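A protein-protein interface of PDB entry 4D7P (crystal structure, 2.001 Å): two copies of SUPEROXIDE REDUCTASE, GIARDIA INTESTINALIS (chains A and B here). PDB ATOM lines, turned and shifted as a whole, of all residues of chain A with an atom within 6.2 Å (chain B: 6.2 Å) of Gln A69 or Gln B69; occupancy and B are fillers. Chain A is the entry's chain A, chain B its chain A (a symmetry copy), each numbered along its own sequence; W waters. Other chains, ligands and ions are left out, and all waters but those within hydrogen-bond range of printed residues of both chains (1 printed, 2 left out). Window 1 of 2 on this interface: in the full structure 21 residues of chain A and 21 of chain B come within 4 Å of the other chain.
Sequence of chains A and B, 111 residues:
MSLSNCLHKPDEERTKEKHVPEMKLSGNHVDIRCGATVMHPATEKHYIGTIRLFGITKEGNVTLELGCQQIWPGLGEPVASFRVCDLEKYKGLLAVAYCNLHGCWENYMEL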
ATOM      1  N   GLY A  49       7.782 -30.013 -10.167  1.00  0.00           N
ATOM      2  CA  GLY A  49       8.776 -29.242  -9.455  1.00  0.00           C
ATOM      3  C   GLY A  49      10.169 -29.463  -9.987  1.00  0.00           C
ATOM      4  O   GLY A  49      10.998 -28.541  -9.970  1.00  0.00           O
ATOM      5  N   THR A  50      10.452 -30.680 -10.449  1.00  0.00           N
ATOM      6  CA  THR A  50      11.781 -30.959 -10.989  1.00  0.00           C
ATOM      7  C   THR A  50      11.715 -31.800 -12.238  1.00  0.00           C
ATOM      8  O   THR A  50      10.822 -32.623 -12.404  1.00  0.00           O
ATOM      9  CB  THR A  50      12.713 -31.708  -9.978  1.00  0.00           C
ATOM     10  OG1 THR A  50      12.122 -32.968  -9.615  1.00  0.00           O
ATOM     11  CG2 THR A  50      12.992 -30.866  -8.724  1.00  0.00           C
ATOM     12  N   ILE A  51      12.689 -31.586 -13.109  1.00  0.00           N
ATOM     13  CA  ILE A  51      12.893 -32.426 -14.267  1.00  0.00           C
ATOM     14  C   ILE A  51      14.353 -32.816 -14.182  1.00  0.00           C
ATOM     15  O   ILE A  51      15.234 -31.950 -14.248  1.00  0.00           O
ATOM     16  CB  ILE A  51      12.583 -31.699 -15.580  1.00  0.00           C
ATOM     17  CG1 ILE A  51      11.088 -31.373 -15.690  1.00  0.00           C
ATOM     18  CG2 ILE A  51      13.043 -32.522 -16.762  1.00  0.00           C
ATOM     19  CD1 ILE A  51      10.773 -30.410 -16.824  1.00  0.00           C
ATOM     20  N   ARG A  52      14.617 -34.098 -13.958  1.00  0.00           N
ATOM     21  CA  ARG A  52      15.991 -34.578 -13.875  1.00  0.00           C
ATOM     22  C   ARG A  52      16.328 -35.389 -15.093  1.00  0.00           C
ATOM     23  O   ARG A  52      15.464 -36.092 -15.616  1.00  0.00           O
ATOM     24  CB  ARG A  52      16.198 -35.427 -12.620  1.00  0.00           C
ATOM     25  CG  ARG A  52      16.098 -34.642 -11.348  1.00  0.00           C
ATOM     26  CD  ARG A  52      15.584 -35.487 -10.216  1.00  0.00           C
ATOM     27  NE  ARG A  52      16.659 -36.134  -9.479  1.00  0.00           N
ATOM     28  CZ  ARG A  52      16.480 -37.222  -8.737  1.00  0.00           C
ATOM     29  NH1 ARG A  52      15.269 -37.763  -8.668  1.00  0.00           N
ATOM     30  NH2 ARG A  52      17.495 -37.782  -8.081  1.00  0.00           N
ATOM     31  N   LEU A  53      17.584 -35.300 -15.526  1.00  0.00           N
ATOM     32  CA  LEU A  53      18.089 -36.105 -16.627  1.00  0.00           C
ATOM     33  C   LEU A  53      19.218 -37.003 -16.137  1.00  0.00           C
ATOM     34  O   LEU A  53      20.173 -36.535 -15.517  1.00  0.00           O
ATOM     35  CB  LEU A  53      18.582 -35.226 -17.790  1.00  0.00           C
ATOM     36  CG  LEU A  53      18.997 -36.004 -19.047  1.00  0.00           C
ATOM     37  CD1 LEU A  53      17.800 -36.765 -19.611  1.00  0.00           C
ATOM     38  CD2 LEU A  53      19.610 -35.097 -20.127  1.00  0.00           C
ATOM     39  N   GLY A  67      21.921 -33.740 -14.235  1.00  0.00           N
ATOM     40  CA  GLY A  67      21.500 -32.467 -13.671  1.00  0.00           C
ATOM     41  C   GLY A  67      20.019 -32.447 -13.335  1.00  0.00           C
ATOM     42  O   GLY A  67      19.319 -33.435 -13.550  1.00  0.00           O
ATOM     43  N   CYS A  68      19.548 -31.325 -12.799  1.00  0.00           N
ATOM     44  CA  CYS A  68      18.189 -31.227 -12.286  1.00  0.00           C
ATOM     45  C   CYS A  68      17.660 -29.828 -12.463  1.00  0.00           C
ATOM     46  O   CYS A  68      18.198 -28.881 -11.871  1.00  0.00           O
ATOM     47  CB  CYS A  68      18.130 -31.618 -10.803  1.00  0.00           C
ATOM     48  SG  CYS A  68      16.485 -31.399 -10.005  1.00  0.00           S
ATOM     49  N   GLN A  69      16.617 -29.700 -13.282  1.00  0.00           N
ATOM     50  CA  GLN A  69      15.888 -28.450 -13.434  1.00  0.00           C
ATOM     51  C   GLN A  69      14.828 -28.342 -12.352  1.00  0.00           C
ATOM     52  O   GLN A  69      13.835 -29.078 -12.357  1.00  0.00           O
ATOM     53  CB  GLN A  69      15.219 -28.345 -14.807  1.00  0.00           C
ATOM     54  CG  GLN A  69      14.351 -27.087 -14.991  1.00  0.00           C
ATOM     55  CD  GLN A  69      15.180 -25.808 -15.019  1.00  0.00           C
ATOM     56  OE1 GLN A  69      15.873 -25.536 -15.990  1.00  0.00           O
ATOM     57  NE2 GLN A  69      15.107 -25.016 -13.948  1.00  0.00           N
ATOM     58  N   GLN A  70      15.037 -27.409 -11.432  1.00  0.00           N
ATOM     59  CA  GLN A  70      14.048 -27.114 -10.412  1.00  0.00           C
ATOM     60  C   GLN A  70      13.220 -25.888 -10.825  1.00  0.00           C
ATOM     61  O   GLN A  70      13.745 -24.906 -11.373  1.00  0.00           O
ATOM     62  CB  GLN A  70      14.742 -26.915  -9.059  1.00  0.00           C
ATOM     63  CG  GLN A  70      13.780 -26.718  -7.884  1.00  0.00           C
ATOM     64  CD  GLN A  70      13.463 -25.253  -7.671  1.00  0.00           C
ATOM     65  OE1 GLN A  70      14.311 -24.401  -7.901  1.00  0.00           O
ATOM     66  NE2 GLN A  70      12.236 -24.950  -7.259  1.00  0.00           N
ATOM     67  N   ILE A  71      11.912 -25.972 -10.612  1.00  0.00           N
ATOM     68  CA  ILE A  71      10.995 -24.917 -11.035  1.00  0.00           C
ATOM     69  C   ILE A  71      10.081 -24.524  -9.885  1.00  0.00           C
ATOM     70  O   ILE A  71       9.451 -25.370  -9.269  1.00  0.00           O
ATOM     71  CB  ILE A  71      10.133 -25.368 -12.224  1.00  0.00           C
ATOM     72  CG1 ILE A  71      11.028 -25.904 -13.344  1.00  0.00           C
ATOM     73  CG2 ILE A  71       9.247 -24.222 -12.721  1.00  0.00           C
ATOM     74  CD1 ILE A  71      10.285 -26.732 -14.367  1.00  0.00           C
ATOM     75  N   VAL A  79       9.450 -27.346 -18.524  1.00  0.00           N
ATOM     76  CA  VAL A  79      10.396 -27.596 -19.591  1.00  0.00           C
ATOM     77  C   VAL A  79      11.805 -27.630 -19.015  1.00  0.00           C
ATOM     78  O   VAL A  79      12.049 -27.151 -17.895  1.00  0.00           O
ATOM     79  CB  VAL A  79      10.322 -26.508 -20.676  1.00  0.00           C
ATOM     80  CG1 VAL A  79       8.904 -26.411 -21.221  1.00  0.00           C
ATOM     81  CG2 VAL A  79      10.726 -25.173 -20.100  1.00  0.00           C
ATOM     82  N   ALA A  80      12.732 -28.182 -19.784  1.00  0.00           N
ATOM     83  CA  ALA A  80      14.135 -28.138 -19.415  1.00  0.00           C
ATOM     84  C   ALA A  80      15.019 -28.412 -20.619  1.00  0.00           C
ATOM     85  O   ALA A  80      14.558 -28.945 -21.630  1.00  0.00           O
ATOM     86  CB  ALA A  80      14.438 -29.163 -18.286  1.00  0.00           C
ATOM     87  N   SER A  81      16.291 -28.038 -20.525  1.00  0.00           N
ATOM     88  CA  SER A  81      17.247 -28.584 -21.475  1.00  0.00           C
ATOM     89  C   SER A  81      18.598 -28.867 -20.833  1.00  0.00           C
ATOM     90  O   SER A  81      18.982 -28.257 -19.835  1.00  0.00           O
ATOM     91  CB  SER A  81      17.403 -27.664 -22.696  1.00  0.00           C
ATOM     92  OG  SER A  81      17.663 -26.324 -22.338  1.00  0.00           O
ATOM     93  N   PHE A  82      19.286 -29.839 -21.414  1.00  0.00           N
ATOM     94  CA  PHE A  82      20.594 -30.267 -20.965  1.00  0.00           C
ATOM     95  C   PHE A  82      21.491 -30.383 -22.159  1.00  0.00           C
ATOM     96  O   PHE A  82      21.028 -30.426 -23.299  1.00  0.00           O
ATOM     97  CB  PHE A  82      20.512 -31.605 -20.257  1.00  0.00           C
ATOM     98  CG  PHE A  82      19.624 -31.592 -19.056  1.00  0.00           C
ATOM     99  CD1 PHE A  82      18.250 -31.642 -19.192  1.00  0.00           C
ATOM    100  CD2 PHE A  82      20.166 -31.524 -17.780  1.00  0.00           C
ATOM    101  CE1 PHE A  82      17.426 -31.634 -18.081  1.00  0.00           C
ATOM    102  CE2 PHE A  82      19.350 -31.520 -16.673  1.00  0.00           C
ATOM    103  CZ  PHE A  82      17.973 -31.570 -16.826  1.00  0.00           C
ATOM    104  N   GLY B  49      27.807 -24.449 -12.251  1.00  0.00           N
ATOM    105  CA  GLY B  49      27.014 -25.400 -11.506  1.00  0.00           C
ATOM    106  C   GLY B  49      25.538 -25.105 -11.576  1.00  0.00           C
ATOM    107  O   GLY B  49      24.713 -26.030 -11.559  1.00  0.00           O
ATOM    108  N   THR B  50      25.183 -23.823 -11.639  1.00  0.00           N
ATOM    109  CA  THR B  50      23.768 -23.466 -11.721  1.00  0.00           C
ATOM    110  C   THR B  50      23.524 -22.349 -12.703  1.00  0.00           C
ATOM    111  O   THR B  50      24.367 -21.481 -12.899  1.00  0.00           O
ATOM    112  CB  THR B  50      23.166 -23.012 -10.348  1.00  0.00           C
ATOM    113  OG1 THR B  50      23.874 -21.858  -9.866  1.00  0.00           O
ATOM    114  CG2 THR B  50      23.205 -24.139  -9.305  1.00  0.00           C
ATOM    115  N   ILE B  51      22.346 -22.380 -13.306  1.00  0.00           N
ATOM    116  CA  ILE B  51      21.867 -21.294 -14.131  1.00  0.00           C
ATOM    117  C   ILE B  51      20.497 -20.985 -13.567  1.00  0.00           C
ATOM    118  O   ILE B  51      19.602 -21.839 -13.600  1.00  0.00           O
ATOM    119  CB  ILE B  51      21.790 -21.675 -15.614  1.00  0.00           C
ATOM    120  CG1 ILE B  51      23.190 -21.915 -16.194  1.00  0.00           C
ATOM    121  CG2 ILE B  51      21.058 -20.608 -16.396  1.00  0.00           C
ATOM    122  CD1 ILE B  51      23.157 -22.567 -17.567  1.00  0.00           C
ATOM    123  N   ARG B  52      20.346 -19.804 -12.981  1.00  0.00           N
ATOM    124  CA  ARG B  52      19.061 -19.403 -12.419  1.00  0.00           C
ATOM    125  C   ARG B  52      18.437 -18.335 -13.272  1.00  0.00           C
ATOM    126  O   ARG B  52      19.152 -17.499 -13.822  1.00  0.00           O
ATOM    127  CB  ARG B  52      19.226 -18.886 -10.990  1.00  0.00           C
ATOM    128  CG  ARG B  52      19.637 -19.950 -10.018  1.00  0.00           C
ATOM    129  CD  ARG B  52      20.462 -19.384  -8.897  1.00  0.00           C
ATOM    130  NE  ARG B  52      19.646 -18.968  -7.766  1.00  0.00           N
ATOM    131  CZ  ARG B  52      20.054 -18.084  -6.860  1.00  0.00           C
ATOM    132  NH1 ARG B  52      21.256 -17.536  -6.990  1.00  0.00           N
ATOM    133  NH2 ARG B  52      19.271 -17.732  -5.843  1.00  0.00           N
ATOM    134  N   LEU B  53      17.108 -18.360 -13.361  1.00  0.00           N
ATOM    135  CA  LEU B  53      16.354 -17.331 -14.060  1.00  0.00           C
ATOM    136  C   LEU B  53      15.429 -16.615 -13.085  1.00  0.00           C
ATOM    137  O   LEU B  53      14.659 -17.250 -12.363  1.00  0.00           O
ATOM    138  CB  LEU B  53      15.538 -17.923 -15.224  1.00  0.00           C
ATOM    139  CG  LEU B  53      14.828 -16.880 -16.099  1.00  0.00           C
ATOM    140  CD1 LEU B  53      15.855 -15.967 -16.764  1.00  0.00           C
ATOM    141  CD2 LEU B  53      13.918 -17.521 -17.161  1.00  0.00           C
ATOM    142  N   GLY B  67      13.226 -20.327 -11.368  1.00  0.00           N
ATOM    143  CA  GLY B  67      13.741 -21.683 -11.260  1.00  0.00           C
ATOM    144  C   GLY B  67      15.256 -21.733 -11.347  1.00  0.00           C
ATOM    145  O   GLY B  67      15.905 -20.701 -11.499  1.00  0.00           O
ATOM    146  N   CYS B  68      15.816 -22.935 -11.242  1.00  0.00           N
ATOM    147  CA  CYS B  68      17.258 -23.108 -11.151  1.00  0.00           C
ATOM    148  C   CYS B  68      17.674 -24.405 -11.793  1.00  0.00           C
ATOM    149  O   CYS B  68      17.283 -25.484 -11.324  1.00  0.00           O
ATOM    150  CB  CYS B  68      17.726 -23.082  -9.690  1.00  0.00           C
ATOM    151  SG  CYS B  68      19.515 -23.431  -9.438  1.00  0.00           S
ATOM    152  N   GLN B  69      18.455 -24.299 -12.867  1.00  0.00           N
ATOM    153  CA  GLN B  69      19.075 -25.451 -13.504  1.00  0.00           C
ATOM    154  C   GLN B  69      20.382 -25.780 -12.804  1.00  0.00           C
ATOM    155  O   GLN B  69      21.361 -25.031 -12.898  1.00  0.00           O
ATOM    156  CB  GLN B  69      19.347 -25.202 -14.989  1.00  0.00           C
ATOM    157  CG  GLN B  69      20.092 -26.349 -15.695  1.00  0.00           C
ATOM    158  CD  GLN B  69      19.244 -27.611 -15.805  1.00  0.00           C
ATOM    159  OE1 GLN B  69      18.308 -27.666 -16.592  1.00  0.00           O
ATOM    160  NE2 GLN B  69      19.575 -28.634 -15.015  1.00  0.00           N
ATOM    161  N   GLN B  70      20.395 -26.912 -12.113  1.00  0.00           N
ATOM    162  CA  GLN B  70      21.611 -27.410 -11.497  1.00  0.00           C
ATOM    163  C   GLN B  70      22.257 -28.473 -12.397  1.00  0.00           C
ATOM    164  O   GLN B  70      21.573 -29.313 -13.004  1.00  0.00           O
ATOM    165  CB  GLN B  70      21.299 -27.951 -10.095  1.00  0.00           C
ATOM    166  CG  GLN B  70      22.533 -28.391  -9.304  1.00  0.00           C
ATOM    167  CD  GLN B  70      22.847 -29.854  -9.541  1.00  0.00           C
ATOM    168  OE1 GLN B  70      21.941 -30.653  -9.733  1.00  0.00           O
ATOM    169  NE2 GLN B  70      24.129 -30.205  -9.557  1.00  0.00           N
ATOM    170  N   ILE B  71      23.577 -28.400 -12.528  1.00  0.00           N
ATOM    171  CA  ILE B  71      24.312 -29.291 -13.422  1.00  0.00           C
ATOM    172  C   ILE B  71      25.486 -29.918 -12.687  1.00  0.00           C
ATOM    173  O   ILE B  71      26.286 -29.224 -12.079  1.00  0.00           O
ATOM    174  CB  ILE B  71      24.838 -28.541 -14.654  1.00  0.00           C
ATOM    175  CG1 ILE B  71      23.694 -27.782 -15.331  1.00  0.00           C
ATOM    176  CG2 ILE B  71      25.520 -29.504 -15.630  1.00  0.00           C
ATOM    177  CD1 ILE B  71      24.163 -26.709 -16.286  1.00  0.00           C
ATOM    178  N   VAL B  79      23.874 -25.090 -20.242  1.00  0.00           N
ATOM    179  CA  VAL B  79      22.686 -24.622 -20.925  1.00  0.00           C
ATOM    180  C   VAL B  79      21.484 -24.775 -20.003  1.00  0.00           C
ATOM    181  O   VAL B  79      21.534 -25.515 -19.006  1.00  0.00           O
ATOM    182  CB  VAL B  79      22.430 -25.416 -22.218  1.00  0.00           C
ATOM    183  CG1 VAL B  79      23.647 -25.333 -23.130  1.00  0.00           C
ATOM    184  CG2 VAL B  79      22.152 -26.862 -21.893  1.00  0.00           C
ATOM    185  N   ALA B  80      20.404 -24.085 -20.339  1.00  0.00           N
ATOM    186  CA  ALA B  80      19.150 -24.263 -19.629  1.00  0.00           C
ATOM    187  C   ALA B  80      17.986 -23.738 -20.451  1.00  0.00           C
ATOM    188  O   ALA B  80      18.177 -22.963 -21.390  1.00  0.00           O
ATOM    189  CB  ALA B  80      19.195 -23.549 -18.249  1.00  0.00           C
ATOM    190  N   SER B  81      16.774 -24.166 -20.112  1.00  0.00           N
ATOM    191  CA  SER B  81      15.617 -23.440 -20.612  1.00  0.00           C
ATOM    192  C   SER B  81      14.497 -23.364 -19.583  1.00  0.00           C
ATOM    193  O   SER B  81      14.374 -24.208 -18.695  1.00  0.00           O
ATOM    194  CB  SER B  81      15.109 -24.045 -21.930  1.00  0.00           C
ATOM    195  OG  SER B  81      14.910 -25.440 -21.847  1.00  0.00           O
ATOM    196  N   PHE B  82      13.712 -22.305 -19.708  1.00  0.00           N
ATOM    197  CA  PHE B  82      12.587 -22.040 -18.836  1.00  0.00           C
ATOM    198  C   PHE B  82      11.407 -21.671 -19.683  1.00  0.00           C
ATOM    199  O   PHE B  82      11.549 -21.341 -20.860  1.00  0.00           O
ATOM    200  CB  PHE B  82      12.900 -20.909 -17.877  1.00  0.00           C
ATOM    201  CG  PHE B  82      14.076 -21.179 -16.997  1.00  0.00           C
ATOM    202  CD1 PHE B  82      15.364 -21.053 -17.480  1.00  0.00           C
ATOM    203  CD2 PHE B  82      13.894 -21.569 -15.677  1.00  0.00           C
ATOM    204  CE1 PHE B  82      16.455 -21.300 -16.666  1.00  0.00           C
ATOM    205  CE2 PHE B  82      14.976 -21.812 -14.864  1.00  0.00           C
ATOM    206  CZ  PHE B  82      16.262 -21.681 -15.363  1.00  0.00           C
HETATM  207  O   HOH W   1      16.839 -26.376 -18.102  1.00  0.00           O
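Printed residues of chain A that touch a printed residue of chain B: Gly A67, Cys A68, Gln A69, Gln A70, Val A79, Ala A80, Ser A81 and Phe A82.
Hydrophobic or aromatic side chains of chain A that line the printed part of chain B: Val A79 and Phe A82.
Among the printed residues, no Asp or Glu carboxylate lies within 4 Å of a Lys or Arg side-chain nitrogen of the other chain.
Of chain B, only Cys B68 (3.4 Å), Gln B69 (3.3 Å), Ser B81 (3.4 Å) and Phe B82 (3.3 Å) come within 4 Å of Gln A69.
Of the printed residues of chain B, Gln A70 touches Gly B67 (3.2 Å) and Cys B68 (2.9 Å).
Of the printed residues of chain B, Phe A82 touches Gln B69 (3.3 Å) and Val B79 (3.6 Å).
Arg B52 touches none of the printed residues of chain A.
Gln B69 touches just these residues of chain A: Cys A68 (3.4 Å), Gln A69 (3.3 Å), Ser A81 (3.4 Å) and Phe A82 (3.3 Å).
The nearest printed residue of chain B that does not touch Phe A82 is Gln B70 (4.8 Å).
Water W1 lies within hydrogen-bond range of the side-chain amide oxygen of Gln A69, the side-chain amide oxygen of Gln B69, the backbone NH of Ser B81 and the backbone NH of Ser A81.
O of Gln B70 touches CA of Gly A67, 3.2 Å away.
Cys B68 touches Cys A68.
Phe B82 touches Gln A69 (CE2 to NE2, 3.3 Å).
Gly B67 touches Gln A70 (CA to O, 3.2 Å).
Val A79 touches Ser B81.
CG2 of Val A79 touches C of Phe B82 (3.6 Å).
Ala A80 touches Ser B81.
O of Ser A81 touches O of Val B79, at 3.8 Å.
Ser A81 touches Ala B80 (OG to C, 3.2 Å).
NE2 of Gln B69 touches CE2 of Phe A82 (3.3 Å).
The side-chain amide oxygen (OE1) of Gln A69 sits close to the backbone carbonyl oxygen (O) of Ser B81 (3.4 Å).
The side-chain hydroxyl of Ser A81 lies within hydrogen-bond range of the side-chain hydroxyl of Ser B81 (2.9 Å).
The backbone carbonyl oxygen of Ser A81 sits close to the side-chain amide oxygen of Gln B69, at 3.4 Å.
The backbone carbonyl oxygen (O) of Cys B68 lies close to the side-chain amide nitrogen (NE2) of Gln A69, at 3.4 Å.
OE1 of Gln A69 lies close to OE1 of Gln B69, at 3.3 Å.
N of Cys A68 sits at hydrogen-bond distance from O of Gln B70, at 2.9 Å.
The backbone carbonyl oxygen of Gln A70 is in hydrogen-bond range of the backbone NH of Cys B68, 2.9 Å away.
O of Cys A68 sits close to NE2 of Gln B69.
O of Ile A51 sits at hydrogen-bond distance from N of Gln A69, at 2.8 Å.
O of Ile B51 is in hydrogen-bond range of N of Gln B69.
N of Leu A53 is in hydrogen-bond range of O of Gly A67 (3.2 Å).
N of Leu B53 lies within hydrogen-bond range of O of Gly B67, at 3.2 Å.
Cys A68 touches its own counterpart, Cys B68.
Cys A68 touches Gln B69, and with the chains exchanged Gln A69 touches Cys B68.
Gln A69 touches Phe B82, and with the chains exchanged Phe A82 touches Gln B69.
Val A79 touches Ser B81, and with the chains exchanged Ser A81 touches Val B79.
14 positions are printed for both chains.
Of the 19 pairs that touch across the chains among the printed residues, 19 have their exchanged pair printed and touching as well.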
